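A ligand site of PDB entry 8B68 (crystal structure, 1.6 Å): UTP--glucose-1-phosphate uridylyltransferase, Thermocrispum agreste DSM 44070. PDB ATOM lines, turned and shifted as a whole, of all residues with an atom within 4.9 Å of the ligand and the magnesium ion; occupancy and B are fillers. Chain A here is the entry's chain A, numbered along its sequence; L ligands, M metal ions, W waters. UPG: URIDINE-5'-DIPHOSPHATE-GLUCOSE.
OD2 of Asp 141 sits at hydrogen-bond distance from N of Gly 213 (2.8 Å).
The side-chain amide nitrogen (NE2) of Gln 110 lies close to the backbone carbonyl oxygen (O) of Gln 112 (3.4 Å).
O of Gly 115 sits at hydrogen-bond distance from NE2 of Gln 110 (3.4 Å).
The backbone carbonyl oxygen (O) of Gly 213 is in hydrogen-bond range of the backbone NH (N) of Leu 138, at 2.9 Å.
The backbone NH (N) of Ala 18 sits at hydrogen-bond distance from the backbone carbonyl oxygen (O) of Val 62 (3.3 Å).
O of Val 62 is in hydrogen-bond range of N of Ala 17.
NE2 of Gln 110 sits close to N of Ala 119 (3.4 Å).
NE2 of Gln 110 sits close to N of Leu 114 (3.4 Å).
The backbone NH of Ala 18 lies within hydrogen-bond range of an oxygen (O2) of the ligand (2.9 Å).
O3C of the ligand lies within hydrogen-bond range of O of Pro 16 (2.8 Å).
An oxygen (O2C) of the ligand is in hydrogen-bond range of the backbone NH (N) of Gly 19 (3.0 Å).
O4' of the ligand lies within hydrogen-bond range of O of Ala 211 (2.7 Å).
An oxygen (O6') of the ligand is in hydrogen-bond range of the side-chain carboxylate (OD2) of Asp 141, at 2.6 Å.
N of Leu 114 sits at hydrogen-bond distance from O4 of the ligand (3.1 Å).
The side-chain amide nitrogen (NE2) of Gln 110 is in hydrogen-bond range of an oxygen (O4) of the ligand (2.9 Å).
O4 of the ligand sits at hydrogen-bond distance from N of Gly 115.
The backbone NH (N) of Ala 17 sits at hydrogen-bond distance from an oxygen (O2) of the ligand.
Merely in contact with the ligand: Glu 34 (3.98 Å), Ala 113 (3.0 Å), Leu 116 (3.7 Å), Ala 119 (3.2 Å), Leu 138 (3.1 Å), Pro 139 (3.4 Å), Ala 212 (3.9 Å), Gly 213 (3.5 Å) and Thr 239 (3.9 Å).
Hydrophobic or aromatic side chains that line the ligand: Pro 16, Ala 18, Ala 113, Leu 116, Ala 119, Leu 138, Pro 139 and Ala 211.
Within 4 Å of the ligand: Pro 16, Ala 17, Ala 18, Gly 19, Glu 34, Gln 110, Ala 113, Leu 114, Gly 115, Leu 116, Ala 119, Leu 138, Pro 139, Asp 141, Ala 211, Ala 212, Gly 213 and Thr 239.
The nearest printed residue that does not touch the ligand is Tyr 215 (4.01 Å).
Water W5 binds the magnesium ion.
Water W4 binds the magnesium ion (2.0 Å).
The magnesium ion is bound by O2B of the ligand, at 2.1 Å.
The magnesium ion is bound by O2A of the ligand (2.4 Å).
The magnesium ion has four donor atoms within binding distance.
No residue comes within 4 Å of the magnesium ion.
Water W6 lies within hydrogen-bond range of O of Gly 19, OE2 of Glu 34 and O2C of the ligand.
Water W3 bridges an oxygen (O3C) of the ligand (2.8 Å) and the backbone NH (N) of Asp 140 (3.0 Å).
Water W7 lies within hydrogen-bond range of O2' of the ligand (2.9 Å), OE1 of Gln 237 (3.0 Å) and N of Thr 239 (3.4 Å).
Water W11 bridges the backbone carbonyl oxygen (O) of Ala 211 (2.7 Å) and an oxygen (O4') of the ligand (3.1 Å).
Water W8 bridges the side-chain hydroxyl of Tyr 215 (2.8 Å) and an oxygen (O3') of the ligand (3.3 Å).
Water W2 lies within hydrogen-bond range of the side-chain carboxylate of Asp 141 (2.6 Å) and an oxygen (O6') of the ligand (3.5 Å).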
ATOM      1  N   PRO A  16      -0.866  -3.322  -1.369  1.00  0.00           N
ATOM      2  CA  PRO A  16      -2.036  -4.135  -1.033  1.00  0.00           C
ATOM      3  C   PRO A  16      -2.163  -4.282   0.476  1.00  0.00           C
ATOM      4  O   PRO A  16      -1.291  -4.865   1.105  1.00  0.00           O
ATOM      5  CB  PRO A  16      -1.784  -5.497  -1.700  1.00  0.00           C
ATOM      6  CG  PRO A  16      -0.615  -5.277  -2.648  1.00  0.00           C
ATOM      7  CD  PRO A  16       0.171  -4.164  -2.008  1.00  0.00           C
ATOM      8  N   ALA A  17      -3.236  -3.703   1.032  1.00  0.00           N
ATOM      9  CA  ALA A  17      -3.428  -3.583   2.495  1.00  0.00           C
ATOM     10  C   ALA A  17      -4.855  -3.935   2.879  1.00  0.00           C
ATOM     11  O   ALA A  17      -5.399  -3.386   3.842  1.00  0.00           O
ATOM     12  CB  ALA A  17      -3.049  -2.197   2.882  1.00  0.00           C
ATOM     13  N   ALA A  18      -5.490  -4.838   2.134  1.00  0.00           N
ATOM     14  CA  ALA A  18      -6.911  -5.090   2.314  1.00  0.00           C
ATOM     15  C   ALA A  18      -7.202  -6.338   3.166  1.00  0.00           C
ATOM     16  O   ALA A  18      -8.367  -6.493   3.563  1.00  0.00           O
ATOM     17  CB  ALA A  18      -7.593  -5.142   0.968  1.00  0.00           C
ATOM     18  N   GLY A  19      -6.187  -7.177   3.479  1.00  0.00           N
ATOM     19  CA  GLY A  19      -6.403  -8.334   4.349  1.00  0.00           C
ATOM     20  C   GLY A  19      -6.394  -7.917   5.825  1.00  0.00           C
ATOM     21  O   GLY A  19      -5.742  -6.925   6.171  1.00  0.00           O
ATOM     22  N   GLU A  34      -1.506  -2.446   9.014  1.00  0.00           N
ATOM     23  CA  GLU A  34      -0.429  -1.650   8.452  1.00  0.00           C
ATOM     24  C   GLU A  34      -0.117  -0.404   9.295  1.00  0.00           C
ATOM     25  O   GLU A  34       0.865   0.268   9.010  1.00  0.00           O
ATOM     26  CB  GLU A  34      -0.782  -1.248   7.024  1.00  0.00           C
ATOM     27  CG  GLU A  34      -0.899  -2.472   6.110  1.00  0.00           C
ATOM     28  CD  GLU A  34      -2.093  -3.377   6.200  1.00  0.00           C
ATOM     29  OE1 GLU A  34      -3.120  -2.983   6.754  1.00  0.00           O
ATOM     30  OE2 GLU A  34      -1.957  -4.537   5.668  1.00  0.00           O
ATOM     31  N   VAL A  62      -4.409  -0.093  -1.480  1.00  0.00           N
ATOM     32  CA  VAL A  62      -5.626  -0.848  -1.627  1.00  0.00           C
ATOM     33  C   VAL A  62      -6.088  -1.317  -0.257  1.00  0.00           C
ATOM     34  O   VAL A  62      -5.362  -2.076   0.380  1.00  0.00           O
ATOM     35  CB  VAL A  62      -5.455  -2.023  -2.587  1.00  0.00           C
ATOM     36  CG1 VAL A  62      -6.811  -2.726  -2.772  1.00  0.00           C
ATOM     37  CG2 VAL A  62      -4.899  -1.560  -3.925  1.00  0.00           C
ATOM     38  N   GLN A 110     -10.997  -2.315  -2.066  1.00  0.00           N
ATOM     39  CA  GLN A 110     -11.316  -3.707  -2.352  1.00  0.00           C
ATOM     40  C   GLN A 110     -12.491  -4.028  -1.423  1.00  0.00           C
ATOM     41  O   GLN A 110     -12.332  -3.999  -0.195  1.00  0.00           O
ATOM     42  CB  GLN A 110     -10.069  -4.580  -2.139  1.00  0.00           C
ATOM     43  CG  GLN A 110      -9.990  -5.903  -2.912  1.00  0.00           C
ATOM     44  CD  GLN A 110      -9.092  -6.931  -2.226  1.00  0.00           C
ATOM     45  OE1 GLN A 110      -8.630  -6.694  -1.122  1.00  0.00           O
ATOM     46  NE2 GLN A 110      -8.845  -8.095  -2.805  1.00  0.00           N
ATOM     47  N   GLN A 112     -14.295  -6.848  -0.896  1.00  0.00           N
ATOM     48  CA  GLN A 112     -13.947  -8.080  -0.180  1.00  0.00           C
ATOM     49  C   GLN A 112     -12.479  -8.473  -0.445  1.00  0.00           C
ATOM     50  O   GLN A 112     -11.972  -8.167  -1.519  1.00  0.00           O
ATOM     51  CB  GLN A 112     -14.787  -9.260  -0.669  1.00  0.00           C
ATOM     52  CG  GLN A 112     -16.278  -9.162  -0.365  1.00  0.00           C
ATOM     53  CD  GLN A 112     -17.002 -10.282  -1.059  1.00  0.00           C
ATOM     54  OE1 GLN A 112     -17.597 -10.097  -2.120  1.00  0.00           O
ATOM     55  NE2 GLN A 112     -16.914 -11.485  -0.497  1.00  0.00           N
ATOM     56  N   ALA A 113     -11.870  -9.215   0.502  1.00  0.00           N
ATOM     57  CA  ALA A 113     -10.492  -9.697   0.379  1.00  0.00           C
ATOM     58  C   ALA A 113     -10.425 -11.001  -0.430  1.00  0.00           C
ATOM     59  O   ALA A 113     -10.312 -12.095   0.113  1.00  0.00           O
ATOM     60  CB  ALA A 113      -9.880  -9.870   1.744  1.00  0.00           C
ATOM     61  N   LEU A 114     -10.419 -10.873  -1.755  1.00  0.00           N
ATOM     62  CA  LEU A 114     -10.428 -12.013  -2.658  1.00  0.00           C
ATOM     63  C   LEU A 114      -8.989 -12.460  -3.010  1.00  0.00           C
ATOM     64  O   LEU A 114      -8.819 -13.363  -3.829  1.00  0.00           O
ATOM     65  CB  LEU A 114     -11.257 -11.621  -3.881  1.00  0.00           C
ATOM     66  CG  LEU A 114     -12.664 -11.081  -3.563  1.00  0.00           C
ATOM     67  CD1 LEU A 114     -13.410 -10.630  -4.818  1.00  0.00           C
ATOM     68  CD2 LEU A 114     -13.458 -12.116  -2.786  1.00  0.00           C
ATOM     69  N   GLY A 115      -7.978 -11.841  -2.378  1.00  0.00           N
ATOM     70  CA  GLY A 115      -6.564 -12.224  -2.425  1.00  0.00           C
ATOM     71  C   GLY A 115      -5.677 -11.131  -3.047  1.00  0.00           C
ATOM     72  O   GLY A 115      -6.149 -10.042  -3.397  1.00  0.00           O
ATOM     73  N   LEU A 116      -4.376 -11.425  -3.174  1.00  0.00           N
ATOM     74  CA  LEU A 116      -3.405 -10.424  -3.594  1.00  0.00           C
ATOM     75  C   LEU A 116      -3.612  -9.994  -5.042  1.00  0.00           C
ATOM     76  O   LEU A 116      -3.525  -8.797  -5.335  1.00  0.00           O
ATOM     77  CB  LEU A 116      -1.994 -10.985  -3.371  1.00  0.00           C
ATOM     78  CG  LEU A 116      -0.827 -10.152  -3.920  1.00  0.00           C
ATOM     79  CD1 LEU A 116      -0.868  -8.727  -3.369  1.00  0.00           C
ATOM     80  CD2 LEU A 116       0.503 -10.816  -3.609  1.00  0.00           C
ATOM     81  N   ALA A 119      -6.387  -7.630  -5.170  1.00  0.00           N
ATOM     82  CA  ALA A 119      -6.007  -6.349  -4.576  1.00  0.00           C
ATOM     83  C   ALA A 119      -5.274  -5.481  -5.586  1.00  0.00           C
ATOM     84  O   ALA A 119      -5.616  -4.306  -5.767  1.00  0.00           O
ATOM     85  CB  ALA A 119      -5.162  -6.554  -3.349  1.00  0.00           C
ATOM     86  N   LEU A 138       4.613  -5.347  -0.720  1.00  0.00           N
ATOM     87  CA  LEU A 138       3.773  -5.988   0.299  1.00  0.00           C
ATOM     88  C   LEU A 138       4.215  -5.466   1.657  1.00  0.00           C
ATOM     89  O   LEU A 138       5.395  -5.563   1.998  1.00  0.00           O
ATOM     90  CB  LEU A 138       3.860  -7.512   0.235  1.00  0.00           C
ATOM     91  CG  LEU A 138       3.563  -8.141  -1.135  1.00  0.00           C
ATOM     92  CD1 LEU A 138       3.452  -9.629  -1.049  1.00  0.00           C
ATOM     93  CD2 LEU A 138       2.323  -7.542  -1.800  1.00  0.00           C
ATOM     94  N   PRO A 139       3.269  -4.908   2.454  1.00  0.00           N
ATOM     95  CA  PRO A 139       3.635  -4.187   3.671  1.00  0.00           C
ATOM     96  C   PRO A 139       4.078  -5.085   4.832  1.00  0.00           C
ATOM     97  O   PRO A 139       4.650  -4.585   5.794  1.00  0.00           O
ATOM     98  CB  PRO A 139       2.361  -3.374   3.944  1.00  0.00           C
ATOM     99  CG  PRO A 139       1.248  -4.238   3.391  1.00  0.00           C
ATOM    100  CD  PRO A 139       1.840  -4.800   2.113  1.00  0.00           C
ATOM    101  N   ASP A 140       3.954  -6.426   4.713  1.00  0.00           N
ATOM    102  CA  ASP A 140       4.484  -7.349   5.710  1.00  0.00           C
ATOM    103  C   ASP A 140       5.945  -7.703   5.500  1.00  0.00           C
ATOM    104  O   ASP A 140       6.570  -8.324   6.365  1.00  0.00           O
ATOM    105  CB  ASP A 140       3.667  -8.620   5.828  1.00  0.00           C
ATOM    106  CG  ASP A 140       2.360  -8.424   6.603  1.00  0.00           C
ATOM    107  OD1 ASP A 140       2.123  -7.296   7.157  1.00  0.00           O
ATOM    108  OD2 ASP A 140       1.625  -9.386   6.636  1.00  0.00           O
ATOM    109  N   ASP A 141       6.494  -7.363   4.327  1.00  0.00           N
ATOM    110  CA  ASP A 141       7.895  -7.610   4.056  1.00  0.00           C
ATOM    111  C   ASP A 141       8.670  -6.314   4.185  1.00  0.00           C
ATOM    112  O   ASP A 141       8.357  -5.328   3.533  1.00  0.00           O
ATOM    113  CB  ASP A 141       8.092  -8.139   2.630  1.00  0.00           C
ATOM    114  CG  ASP A 141       7.824  -9.608   2.454  1.00  0.00           C
ATOM    115  OD1 ASP A 141       7.972 -10.407   3.436  1.00  0.00           O
ATOM    116  OD2 ASP A 141       7.370  -9.952   1.351  1.00  0.00           O
ATOM    117  N   MET A 196       7.235 -20.805 -11.233  1.00  0.00           N
ATOM    118  CA  MET A 196       7.361 -20.829  -9.782  1.00  0.00           C
ATOM    119  C   MET A 196       6.676 -22.097  -9.250  1.00  0.00           C
ATOM    120  O   MET A 196       5.720 -22.561  -9.870  1.00  0.00           O
ATOM    121  CB  MET A 196       6.737 -19.578  -9.155  1.00  0.00           C
ATOM    122  CG  MET A 196       7.329 -19.235  -7.806  1.00  0.00           C
ATOM    123  SD  MET A 196       6.190 -18.288  -6.775  1.00  0.00           S
ATOM    124  CE  MET A 196       5.145 -19.684  -6.350  1.00  0.00           C
ATOM    125  N   ALA A 211      10.268 -16.309  -3.403  1.00  0.00           N
ATOM    126  CA  ALA A 211       9.613 -15.078  -3.784  1.00  0.00           C
ATOM    127  C   ALA A 211       9.390 -14.140  -2.591  1.00  0.00           C
ATOM    128  O   ALA A 211       8.846 -14.592  -1.565  1.00  0.00           O
ATOM    129  CB  ALA A 211       8.318 -15.424  -4.485  1.00  0.00           C
ATOM    130  N   ALA A 212       9.841 -12.892  -2.711  1.00  0.00           N
ATOM    131  CA  ALA A 212       9.709 -11.781  -1.772  1.00  0.00           C
ATOM    132  C   ALA A 212       8.662 -10.794  -2.264  1.00  0.00           C
ATOM    133  O   ALA A 212       8.462 -10.651  -3.493  1.00  0.00           O
ATOM    134  CB  ALA A 212      11.018 -11.098  -1.590  1.00  0.00           C
ATOM    135  N   GLY A 213       8.091  -9.983  -1.324  1.00  0.00           N
ATOM    136  CA  GLY A 213       6.982  -9.098  -1.636  1.00  0.00           C
ATOM    137  C   GLY A 213       7.390  -7.759  -2.233  1.00  0.00           C
ATOM    138  O   GLY A 213       6.975  -6.705  -1.755  1.00  0.00           O
ATOM    139  N   TYR A 215       7.744  -6.044  -6.345  1.00  0.00           N
ATOM    140  CA  TYR A 215       7.435  -6.321  -7.761  1.00  0.00           C
ATOM    141  C   TYR A 215       7.529  -5.028  -8.561  1.00  0.00           C
ATOM    142  O   TYR A 215       7.163  -3.954  -8.081  1.00  0.00           O
ATOM    143  CB  TYR A 215       6.005  -6.826  -7.982  1.00  0.00           C
ATOM    144  CG  TYR A 215       5.521  -7.919  -7.070  1.00  0.00           C
ATOM    145  CD1 TYR A 215       5.188  -7.656  -5.728  1.00  0.00           C
ATOM    146  CD2 TYR A 215       5.378  -9.211  -7.554  1.00  0.00           C
ATOM    147  CE1 TYR A 215       4.764  -8.683  -4.913  1.00  0.00           C
ATOM    148  CE2 TYR A 215       4.989 -10.251  -6.723  1.00  0.00           C
ATOM    149  CZ  TYR A 215       4.701  -9.970  -5.408  1.00  0.00           C
ATOM    150  OH  TYR A 215       4.228 -11.001  -4.600  1.00  0.00           O
ATOM    151  N   GLN A 237      -4.710 -15.366  -7.648  1.00  0.00           N
ATOM    152  CA  GLN A 237      -3.301 -15.329  -7.231  1.00  0.00           C
ATOM    153  C   GLN A 237      -2.496 -14.500  -8.240  1.00  0.00           C
ATOM    154  O   GLN A 237      -2.567 -14.806  -9.438  1.00  0.00           O
ATOM    155  CB  GLN A 237      -2.607 -16.714  -7.217  1.00  0.00           C
ATOM    156  CG  GLN A 237      -2.991 -17.694  -6.104  1.00  0.00           C
ATOM    157  CD  GLN A 237      -2.905 -17.120  -4.717  1.00  0.00           C
ATOM    158  OE1 GLN A 237      -1.925 -16.469  -4.336  1.00  0.00           O
ATOM    159  NE2 GLN A 237      -3.976 -17.307  -3.962  1.00  0.00           N
ATOM    160  N   THR A 239       0.622 -14.827  -8.620  1.00  0.00           N
ATOM    161  CA  THR A 239       1.586 -15.754  -9.233  1.00  0.00           C
ATOM    162  C   THR A 239       1.008 -16.445 -10.456  1.00  0.00           C
ATOM    163  O   THR A 239       1.733 -16.787 -11.400  1.00  0.00           O
ATOM    164  CB  THR A 239       2.118 -16.838  -8.281  1.00  0.00           C
ATOM    165  OG1 THR A 239       1.018 -17.740  -8.102  1.00  0.00           O
ATOM    166  CG2 THR A 239       2.702 -16.256  -7.020  1.00  0.00           C
HETATM  167  N1  UPG L   1      -4.068  -8.581   0.487  1.00  0.00           N
HETATM  168  C2  UPG L   1      -4.944  -7.659  -0.019  1.00  0.00           C
HETATM  169  N3  UPG L   1      -6.172  -8.169  -0.382  1.00  0.00           N
HETATM  170  C4  UPG L   1      -6.590  -9.476  -0.285  1.00  0.00           C
HETATM  171  C5  UPG L   1      -5.632 -10.365   0.292  1.00  0.00           C
HETATM  172  C6  UPG L   1      -4.431  -9.898   0.656  1.00  0.00           C
HETATM  173  O2  UPG L   1      -4.675  -6.483  -0.165  1.00  0.00           O
HETATM  174  O4  UPG L   1      -7.687  -9.793  -0.723  1.00  0.00           O
HETATM  175  C1C UPG L   1      -2.762  -8.092   0.944  1.00  0.00           C
HETATM  176  C2C UPG L   1      -2.497  -8.438   2.409  1.00  0.00           C
HETATM  177  O2C UPG L   1      -3.198  -7.469   3.151  1.00  0.00           O
HETATM  178  C3C UPG L   1      -0.971  -8.335   2.442  1.00  0.00           C
HETATM  179  C4C UPG L   1      -0.546  -8.717   1.006  1.00  0.00           C
HETATM  180  O4C UPG L   1      -1.745  -8.693   0.184  1.00  0.00           O
HETATM  181  O3C UPG L   1      -0.655  -7.009   2.835  1.00  0.00           O
HETATM  182  C5C UPG L   1       0.009 -10.105   0.850  1.00  0.00           C
HETATM  183  O5C UPG L   1      -0.986 -11.012   1.329  1.00  0.00           O
HETATM  184  PA  UPG L   1      -0.543 -12.227   2.272  1.00  0.00           P
HETATM  185  O1A UPG L   1      -1.736 -13.036   2.647  1.00  0.00           O
HETATM  186  O2A UPG L   1       0.265 -11.684   3.410  1.00  0.00           O
HETATM  187  O3A UPG L   1       0.389 -13.022   1.225  1.00  0.00           O
HETATM  188  PB  UPG L   1       1.471 -14.192   1.460  1.00  0.00           P
HETATM  189  O1B UPG L   1       0.718 -15.452   1.808  1.00  0.00           O
HETATM  190  O2B UPG L   1       2.577 -13.720   2.378  1.00  0.00           O
HETATM  191  O3B UPG L   1       2.130 -14.382   0.004  1.00  0.00           O
HETATM  192  C1' UPG L   1       2.425 -13.322  -0.877  1.00  0.00           C
HETATM  193  C2' UPG L   1       2.694 -13.876  -2.271  1.00  0.00           C
HETATM  194  C3' UPG L   1       3.930 -14.788  -2.242  1.00  0.00           C
HETATM  195  C4' UPG L   1       5.128 -13.999  -1.751  1.00  0.00           C
HETATM  196  C5' UPG L   1       4.835 -13.338  -0.383  1.00  0.00           C
HETATM  197  C6' UPG L   1       5.849 -12.294   0.031  1.00  0.00           C
HETATM  198  O2' UPG L   1       1.521 -14.517  -2.746  1.00  0.00           O
HETATM  199  O3' UPG L   1       4.238 -15.360  -3.528  1.00  0.00           O
HETATM  200  O4' UPG L   1       6.160 -14.951  -1.589  1.00  0.00           O
HETATM  201  O5' UPG L   1       3.555 -12.642  -0.383  1.00  0.00           O
HETATM  202  O6' UPG L   1       5.545 -11.856   1.353  1.00  0.00           O
HETATM  203 MG    MG M   1       2.566 -12.134   3.684  1.00  0.00          MG
HETATM  204  O   HOH W   1      -6.333 -11.836   2.924  1.00  0.00           O
HETATM  205  O   HOH W   2       8.363 -12.949   3.037  1.00  0.00           O
HETATM  206  O   HOH W   3       1.917  -8.009   3.154  1.00  0.00           O
HETATM  207  O   HOH W   4       2.997 -10.763   2.311  1.00  0.00           O
HETATM  208  O   HOH W   5       2.106 -11.926   5.606  1.00  0.00           O
HETATM  209  O   HOH W   6      -3.308  -6.709   5.694  1.00  0.00           O
HETATM  210  O   HOH W   7       0.140 -14.495  -5.266  1.00  0.00           O
HETATM  211  O   HOH W   8       3.334 -13.301  -5.894  1.00  0.00           O
HETATM  212  O   HOH W   9       5.322 -13.433   3.707  1.00  0.00           O
HETATM  213  O   HOH W  10      -0.024  -6.427   5.794  1.00  0.00           O
HETATM  214  O   HOH W  11       7.828 -14.271   0.886  1.00  0.00           O
HETATM  215  O   HOH W  12       5.196 -17.625  -2.995  1.00  0.00           O
